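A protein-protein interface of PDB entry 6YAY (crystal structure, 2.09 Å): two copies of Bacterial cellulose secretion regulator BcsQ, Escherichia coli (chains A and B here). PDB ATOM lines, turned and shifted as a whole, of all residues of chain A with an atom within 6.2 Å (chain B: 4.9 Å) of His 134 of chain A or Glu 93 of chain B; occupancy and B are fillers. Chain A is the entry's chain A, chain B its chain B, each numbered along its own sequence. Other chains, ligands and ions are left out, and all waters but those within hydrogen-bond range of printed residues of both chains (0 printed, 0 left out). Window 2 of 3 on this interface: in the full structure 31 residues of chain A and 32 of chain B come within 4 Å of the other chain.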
ATOM      1  N   ARG A 127      13.066   4.519 -15.168  1.00  0.00           N
ATOM      2  CA  ARG A 127      12.613   5.265 -13.994  1.00  0.00           C
ATOM      3  C   ARG A 127      11.950   4.286 -13.030  1.00  0.00           C
ATOM      4  O   ARG A 127      10.726   4.155 -12.951  1.00  0.00           O
ATOM      5  CB  ARG A 127      11.672   6.395 -14.403  1.00  0.00           C
ATOM      6  CG  ARG A 127      11.021   7.168 -13.245  1.00  0.00           C
ATOM      7  CD  ARG A 127      11.994   8.114 -12.557  1.00  0.00           C
ATOM      8  NE  ARG A 127      12.822   7.448 -11.554  1.00  0.00           N
ATOM      9  CZ  ARG A 127      13.946   7.959 -11.056  1.00  0.00           C
ATOM     10  NH1 ARG A 127      14.385   9.137 -11.473  1.00  0.00           N
ATOM     11  NH2 ARG A 127      14.636   7.287 -10.146  1.00  0.00           N
ATOM     12  N   ASP A 128      12.793   3.564 -12.303  1.00  0.00           N
ATOM     13  CA  ASP A 128      12.350   2.730 -11.195  1.00  0.00           C
ATOM     14  C   ASP A 128      13.528   2.558 -10.245  1.00  0.00           C
ATOM     15  O   ASP A 128      14.592   3.161 -10.424  1.00  0.00           O
ATOM     16  CB  ASP A 128      11.803   1.378 -11.672  1.00  0.00           C
ATOM     17  CG  ASP A 128      12.811   0.582 -12.485  1.00  0.00           C
ATOM     18  OD1 ASP A 128      13.878   0.207 -11.949  1.00  0.00           O
ATOM     19  OD2 ASP A 128      12.521   0.312 -13.668  1.00  0.00           O
ATOM     20  N   ALA A 129      13.332   1.720  -9.235  1.00  0.00           N
ATOM     21  CA  ALA A 129      14.331   1.479  -8.210  1.00  0.00           C
ATOM     22  C   ALA A 129      14.597  -0.008  -8.063  1.00  0.00           C
ATOM     23  O   ALA A 129      14.842  -0.505  -6.960  1.00  0.00           O
ATOM     24  CB  ALA A 129      13.899   2.089  -6.878  1.00  0.00           C
ATOM     25  N   SER A 130      14.540  -0.740  -9.177  1.00  0.00           N
ATOM     26  CA  SER A 130      14.767  -2.173  -9.140  1.00  0.00           C
ATOM     27  C   SER A 130      16.230  -2.470  -8.816  1.00  0.00           C
ATOM     28  O   SER A 130      17.082  -1.579  -8.763  1.00  0.00           O
ATOM     29  CB  SER A 130      14.381  -2.812 -10.469  1.00  0.00           C
ATOM     30  OG  SER A 130      15.342  -2.524 -11.472  1.00  0.00           O
ATOM     31  N   GLN A 131      16.513  -3.754  -8.589  1.00  0.00           N
ATOM     32  CA  GLN A 131      17.872  -4.165  -8.257  1.00  0.00           C
ATOM     33  C   GLN A 131      18.813  -3.975  -9.441  1.00  0.00           C
ATOM     34  O   GLN A 131      19.916  -3.435  -9.292  1.00  0.00           O
ATOM     35  CB  GLN A 131      17.879  -5.624  -7.796  1.00  0.00           C
ATOM     36  CG  GLN A 131      17.073  -5.883  -6.534  1.00  0.00           C
ATOM     37  CD  GLN A 131      17.148  -7.334  -6.092  1.00  0.00           C
ATOM     38  OE1 GLN A 131      17.601  -8.200  -6.843  1.00  0.00           O
ATOM     39  NE2 GLN A 131      16.706  -7.604  -4.869  1.00  0.00           N
ATOM     40  N   ILE A 132      18.394  -4.414 -10.630  1.00  0.00           N
ATOM     41  CA  ILE A 132      19.253  -4.309 -11.806  1.00  0.00           C
ATOM     42  C   ILE A 132      19.520  -2.849 -12.156  1.00  0.00           C
ATOM     43  O   ILE A 132      20.606  -2.507 -12.639  1.00  0.00           O
ATOM     44  CB  ILE A 132      18.629  -5.077 -12.990  1.00  0.00           C
ATOM     45  CG1 ILE A 132      19.550  -5.016 -14.210  1.00  0.00           C
ATOM     46  CG2 ILE A 132      17.241  -4.539 -13.323  1.00  0.00           C
ATOM     47  CD1 ILE A 132      20.924  -5.584 -13.947  1.00  0.00           C
ATOM     48  N   THR A 133      18.550  -1.965 -11.905  1.00  0.00           N
ATOM     49  CA  THR A 133      18.742  -0.545 -12.190  1.00  0.00           C
ATOM     50  C   THR A 133      19.800   0.062 -11.276  1.00  0.00           C
ATOM     51  O   THR A 133      20.694   0.783 -11.738  1.00  0.00           O
ATOM     52  CB  THR A 133      17.416   0.200 -12.044  1.00  0.00           C
ATOM     53  OG1 THR A 133      16.495  -0.271 -13.033  1.00  0.00           O
ATOM     54  CG2 THR A 133      17.623   1.696 -12.211  1.00  0.00           C
ATOM     55  N   HIS A 134      19.709  -0.215  -9.974  1.00  0.00           N
ATOM     56  CA  HIS A 134      20.703   0.284  -9.028  1.00  0.00           C
ATOM     57  C   HIS A 134      22.076  -0.313  -9.302  1.00  0.00           C
ATOM     58  O   HIS A 134      23.099   0.361  -9.132  1.00  0.00           O
ATOM     59  CB  HIS A 134      20.267  -0.028  -7.596  1.00  0.00           C
ATOM     60  CG  HIS A 134      19.074   0.753  -7.143  1.00  0.00           C
ATOM     61  ND1 HIS A 134      18.358   0.430  -6.011  1.00  0.00           N
ATOM     62  CD2 HIS A 134      18.472   1.846  -7.669  1.00  0.00           C
ATOM     63  CE1 HIS A 134      17.366   1.289  -5.860  1.00  0.00           C
ATOM     64  NE2 HIS A 134      17.414   2.159  -6.852  1.00  0.00           N
ATOM     65  N   GLN A 135      22.119  -1.579  -9.722  1.00  0.00           N
ATOM     66  CA  GLN A 135      23.397  -2.222 -10.015  1.00  0.00           C
ATOM     67  C   GLN A 135      24.077  -1.567 -11.211  1.00  0.00           C
ATOM     68  O   GLN A 135      25.275  -1.266 -11.170  1.00  0.00           O
ATOM     69  CB  GLN A 135      23.186  -3.715 -10.265  1.00  0.00           C
ATOM     70  CG  GLN A 135      22.885  -4.523  -9.016  1.00  0.00           C
ATOM     71  CD  GLN A 135      22.486  -5.949  -9.334  1.00  0.00           C
ATOM     72  OE1 GLN A 135      22.206  -6.285 -10.484  1.00  0.00           O
ATOM     73  NE2 GLN A 135      22.456  -6.798  -8.314  1.00  0.00           N
ATOM     74  N   LEU A 136      23.322  -1.338 -12.286  1.00  0.00           N
ATOM     75  CA  LEU A 136      23.889  -0.687 -13.460  1.00  0.00           C
ATOM     76  C   LEU A 136      24.307   0.743 -13.147  1.00  0.00           C
ATOM     77  O   LEU A 136      25.334   1.220 -13.647  1.00  0.00           O
ATOM     78  CB  LEU A 136      22.882  -0.727 -14.606  1.00  0.00           C
ATOM     79  CG  LEU A 136      22.646  -2.128 -15.174  1.00  0.00           C
ATOM     80  CD1 LEU A 136      21.352  -2.186 -15.962  1.00  0.00           C
ATOM     81  CD2 LEU A 136      23.819  -2.535 -16.050  1.00  0.00           C
ATOM     82  N   LEU A 137      23.532   1.439 -12.309  1.00  0.00           N
ATOM     83  CA  LEU A 137      23.908   2.783 -11.883  1.00  0.00           C
ATOM     84  C   LEU A 137      25.241   2.791 -11.145  1.00  0.00           C
ATOM     85  O   LEU A 137      25.976   3.783 -11.206  1.00  0.00           O
ATOM     86  CB  LEU A 137      22.816   3.380 -10.998  1.00  0.00           C
ATOM     87  CG  LEU A 137      21.937   4.451 -11.638  1.00  0.00           C
ATOM     88  CD1 LEU A 137      20.882   4.925 -10.650  1.00  0.00           C
ATOM     89  CD2 LEU A 137      22.796   5.612 -12.118  1.00  0.00           C
ATOM     90  N   SER A 138      25.563   1.705 -10.436  1.00  0.00           N
ATOM     91  CA  SER A 138      26.851   1.627  -9.754  1.00  0.00           C
ATOM     92  C   SER A 138      28.002   1.492 -10.743  1.00  0.00           C
ATOM     93  O   SER A 138      29.117   1.942 -10.462  1.00  0.00           O
ATOM     94  CB  SER A 138      26.859   0.456  -8.771  1.00  0.00           C
ATOM     95  OG  SER A 138      25.824   0.594  -7.815  1.00  0.00           O
ATOM     96  N   LEU A 139      27.748   0.878 -11.900  1.00  0.00           N
ATOM     97  CA  LEU A 139      28.773   0.733 -12.927  1.00  0.00           C
ATOM     98  C   LEU A 139      29.092   2.047 -13.627  1.00  0.00           C
ATOM     99  O   LEU A 139      30.136   2.145 -14.279  1.00  0.00           O
ATOM    100  CB  LEU A 139      28.329  -0.298 -13.967  1.00  0.00           C
ATOM    101  CG  LEU A 139      28.697  -1.771 -13.773  1.00  0.00           C
ATOM    102  CD1 LEU A 139      28.288  -2.277 -12.406  1.00  0.00           C
ATOM    103  CD2 LEU A 139      28.043  -2.597 -14.863  1.00  0.00           C
ATOM    104  N   GLN A 160      12.686  13.365  -4.279  1.00  0.00           N
ATOM    105  CA  GLN A 160      13.246  12.080  -4.665  1.00  0.00           C
ATOM    106  C   GLN A 160      14.751  12.202  -4.865  1.00  0.00           C
ATOM    107  O   GLN A 160      15.271  13.274  -5.189  1.00  0.00           O
ATOM    108  CB  GLN A 160      12.577  11.536  -5.933  1.00  0.00           C
ATOM    109  CG  GLN A 160      13.139  12.066  -7.231  1.00  0.00           C
ATOM    110  CD  GLN A 160      12.373  11.558  -8.437  1.00  0.00           C
ATOM    111  OE1 GLN A 160      11.139  11.554  -8.446  1.00  0.00           O
ATOM    112  NE2 GLN A 160      13.097  11.122  -9.464  1.00  0.00           N
ATOM    113  N   ALA A 161      15.448  11.091  -4.652  1.00  0.00           N
ATOM    114  CA  ALA A 161      16.899  11.069  -4.725  1.00  0.00           C
ATOM    115  C   ALA A 161      17.360  10.814  -6.152  1.00  0.00           C
ATOM    116  O   ALA A 161      16.804   9.968  -6.859  1.00  0.00           O
ATOM    117  CB  ALA A 161      17.469  10.000  -3.793  1.00  0.00           C
ATOM    118  N   ILE B  89      13.598   8.229   1.723  1.00  0.00           N
ATOM    119  CA  ILE B  89      14.492   7.890   0.619  1.00  0.00           C
ATOM    120  C   ILE B  89      14.804   6.398   0.618  1.00  0.00           C
ATOM    121  O   ILE B  89      14.834   5.755  -0.439  1.00  0.00           O
ATOM    122  CB  ILE B  89      15.773   8.742   0.692  1.00  0.00           C
ATOM    123  CG1 ILE B  89      15.446  10.211   0.402  1.00  0.00           C
ATOM    124  CG2 ILE B  89      16.829   8.220  -0.276  1.00  0.00           C
ATOM    125  CD1 ILE B  89      16.664  11.106   0.326  1.00  0.00           C
ATOM    126  N   GLU B  90      15.022   5.819   1.801  1.00  0.00           N
ATOM    127  CA  GLU B  90      15.294   4.387   1.882  1.00  0.00           C
ATOM    128  C   GLU B  90      14.114   3.571   1.364  1.00  0.00           C
ATOM    129  O   GLU B  90      14.304   2.565   0.668  1.00  0.00           O
ATOM    130  CB  GLU B  90      15.630   4.001   3.322  1.00  0.00           C
ATOM    131  CG  GLU B  90      16.108   2.567   3.500  1.00  0.00           C
ATOM    132  CD  GLU B  90      14.977   1.590   3.775  1.00  0.00           C
ATOM    133  OE1 GLU B  90      13.847   2.042   4.063  1.00  0.00           O
ATOM    134  OE2 GLU B  90      15.223   0.366   3.705  1.00  0.00           O
ATOM    135  N   GLU B  91      12.887   3.992   1.688  1.00  0.00           N
ATOM    136  CA  GLU B  91      11.710   3.279   1.205  1.00  0.00           C
ATOM    137  C   GLU B  91      11.524   3.470  -0.296  1.00  0.00           C
ATOM    138  O   GLU B  91      11.120   2.536  -0.999  1.00  0.00           O
ATOM    139  CB  GLU B  91      10.463   3.740   1.961  1.00  0.00           C
ATOM    140  CG  GLU B  91      10.534   3.522   3.463  1.00  0.00           C
ATOM    141  CD  GLU B  91       9.311   4.049   4.192  1.00  0.00           C
ATOM    142  OE1 GLU B  91       8.636   3.253   4.879  1.00  0.00           O
ATOM    143  OE2 GLU B  91       9.025   5.260   4.075  1.00  0.00           O
ATOM    144  N   GLN B  92      11.812   4.671  -0.804  1.00  0.00           N
ATOM    145  CA  GLN B  92      11.692   4.921  -2.238  1.00  0.00           C
ATOM    146  C   GLN B  92      12.611   4.008  -3.040  1.00  0.00           C
ATOM    147  O   GLN B  92      12.217   3.483  -4.087  1.00  0.00           O
ATOM    148  CB  GLN B  92      12.008   6.384  -2.551  1.00  0.00           C
ATOM    149  CG  GLN B  92      11.079   7.395  -1.911  1.00  0.00           C
ATOM    150  CD  GLN B  92      11.465   8.820  -2.254  1.00  0.00           C
ATOM    151  OE1 GLN B  92      11.912   9.100  -3.362  1.00  0.00           O
ATOM    152  NE2 GLN B  92      11.298   9.728  -1.299  1.00  0.00           N
ATOM    153  N   GLU B  93      13.839   3.811  -2.571  1.00  0.00           N
ATOM    154  CA  GLU B  93      14.829   3.043  -3.311  1.00  0.00           C
ATOM    155  C   GLU B  93      14.801   1.556  -2.983  1.00  0.00           C
ATOM    156  O   GLU B  93      15.683   0.820  -3.435  1.00  0.00           O
ATOM    157  CB  GLU B  93      16.228   3.611  -3.058  1.00  0.00           C
ATOM    158  CG  GLU B  93      16.404   5.044  -3.551  1.00  0.00           C
ATOM    159  CD  GLU B  93      16.109   5.194  -5.035  1.00  0.00           C
ATOM    160  OE1 GLU B  93      16.543   4.330  -5.826  1.00  0.00           O
ATOM    161  OE2 GLU B  93      15.435   6.175  -5.410  1.00  0.00           O
ATOM    162  N   ASN B  94      13.817   1.097  -2.212  1.00  0.00           N
ATOM    163  CA  ASN B  94      13.651  -0.325  -1.903  1.00  0.00           C
ATOM    164  C   ASN B  94      12.172  -0.680  -1.940  1.00  0.00           C
ATOM    165  O   ASN B  94      11.580  -1.057  -0.920  1.00  0.00           O
ATOM    166  CB  ASN B  94      14.264  -0.665  -0.544  1.00  0.00           C
ATOM    167  CG  ASN B  94      15.777  -0.742  -0.591  1.00  0.00           C
ATOM    168  OD1 ASN B  94      16.346  -1.769  -0.964  1.00  0.00           O
ATOM    169  ND2 ASN B  94      16.437   0.345  -0.207  1.00  0.00           N
ATOM    170  N   PRO B  95      11.543  -0.592  -3.116  1.00  0.00           N
ATOM    171  CA  PRO B  95      10.098  -0.863  -3.194  1.00  0.00           C
ATOM    172  C   PRO B  95       9.719  -2.284  -2.811  1.00  0.00           C
ATOM    173  O   PRO B  95       8.573  -2.511  -2.402  1.00  0.00           O
ATOM    174  CB  PRO B  95       9.766  -0.571  -4.662  1.00  0.00           C
ATOM    175  CG  PRO B  95      11.058  -0.787  -5.383  1.00  0.00           C
ATOM    176  CD  PRO B  95      12.125  -0.316  -4.443  1.00  0.00           C
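The side-chain carboxylate (OE1) of Glu 93 of chain B sits at hydrogen-bond distance from a ring nitrogen (NE2) of His 134 of chain A, 2.6 Å away.
The side-chain amide nitrogen (NE2) of Gln 160 of chain A lies close to the guanidinium group (NH1) of Arg 127 of chain A. O of His 134 of chain A is in hydrogen-bond range of OG of Ser 138 of chain A (3.0 Å).
Among the printed residues, pairs that only touch across the chains: Ala 129 of chain A with Gln 92 of chain B (3.5 Å), Ala 129 of chain A with Glu 93 of chain B (3.6 Å), Ala 129 of chain A with Pro 95 of chain B (3.7 Å), Gln 160 of chain A with Gln 92 of chain B (3.5 Å) and Ala 161 of chain A with Ile 89 of chain B (3.99 Å).
Of the printed residues of chain B, Ala 129 of chain A touches Gln 92 (3.5 Å), Glu 93 (3.6 Å) and Pro 95 (3.7 Å). Of chain B, only Glu 93 (2.6 Å) comes within 4 Å of His 134 of chain A. Leu 136 of chain A touches none of the printed residues of chain B. Of the printed residues of chain B, Ala 161 of chain A touches Ile 89 (3.99 Å). Printed residues of chain A within 4 Å of Ile 89 of chain B: Ala 161. Of the printed residues of chain A, Gln 92 of chain B touches Ala 129 and Gln 160. Of the printed residues of chain A, Glu 93 of chain B touches Ala 129 and His 134. Of the printed residues of chain A, Pro 95 of chain B touches Ala 129 (3.7 Å). The nearest residue of chain A that does not touch Glu 93 of chain B is Ala 161 of chain A (4.3 Å).
Hydrophobic or aromatic side chains of chain A that line the printed part of chain B: Ala 129, His 134 and Ala 161. Of the 7 printed residues of chain B, 4 touch a printed residue of chain A. Hydrophobic or aromatic side chains of chain B within 4 Å of the printed part of chain A: Ile 89 and Pro 95. Among the printed residues, 6 pairs touch across the chains. Among the printed residues, no Asp or Glu carboxylate lies within 4 Å of a Lys or Arg side-chain nitrogen of the other chain.
No position is printed for both chains.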
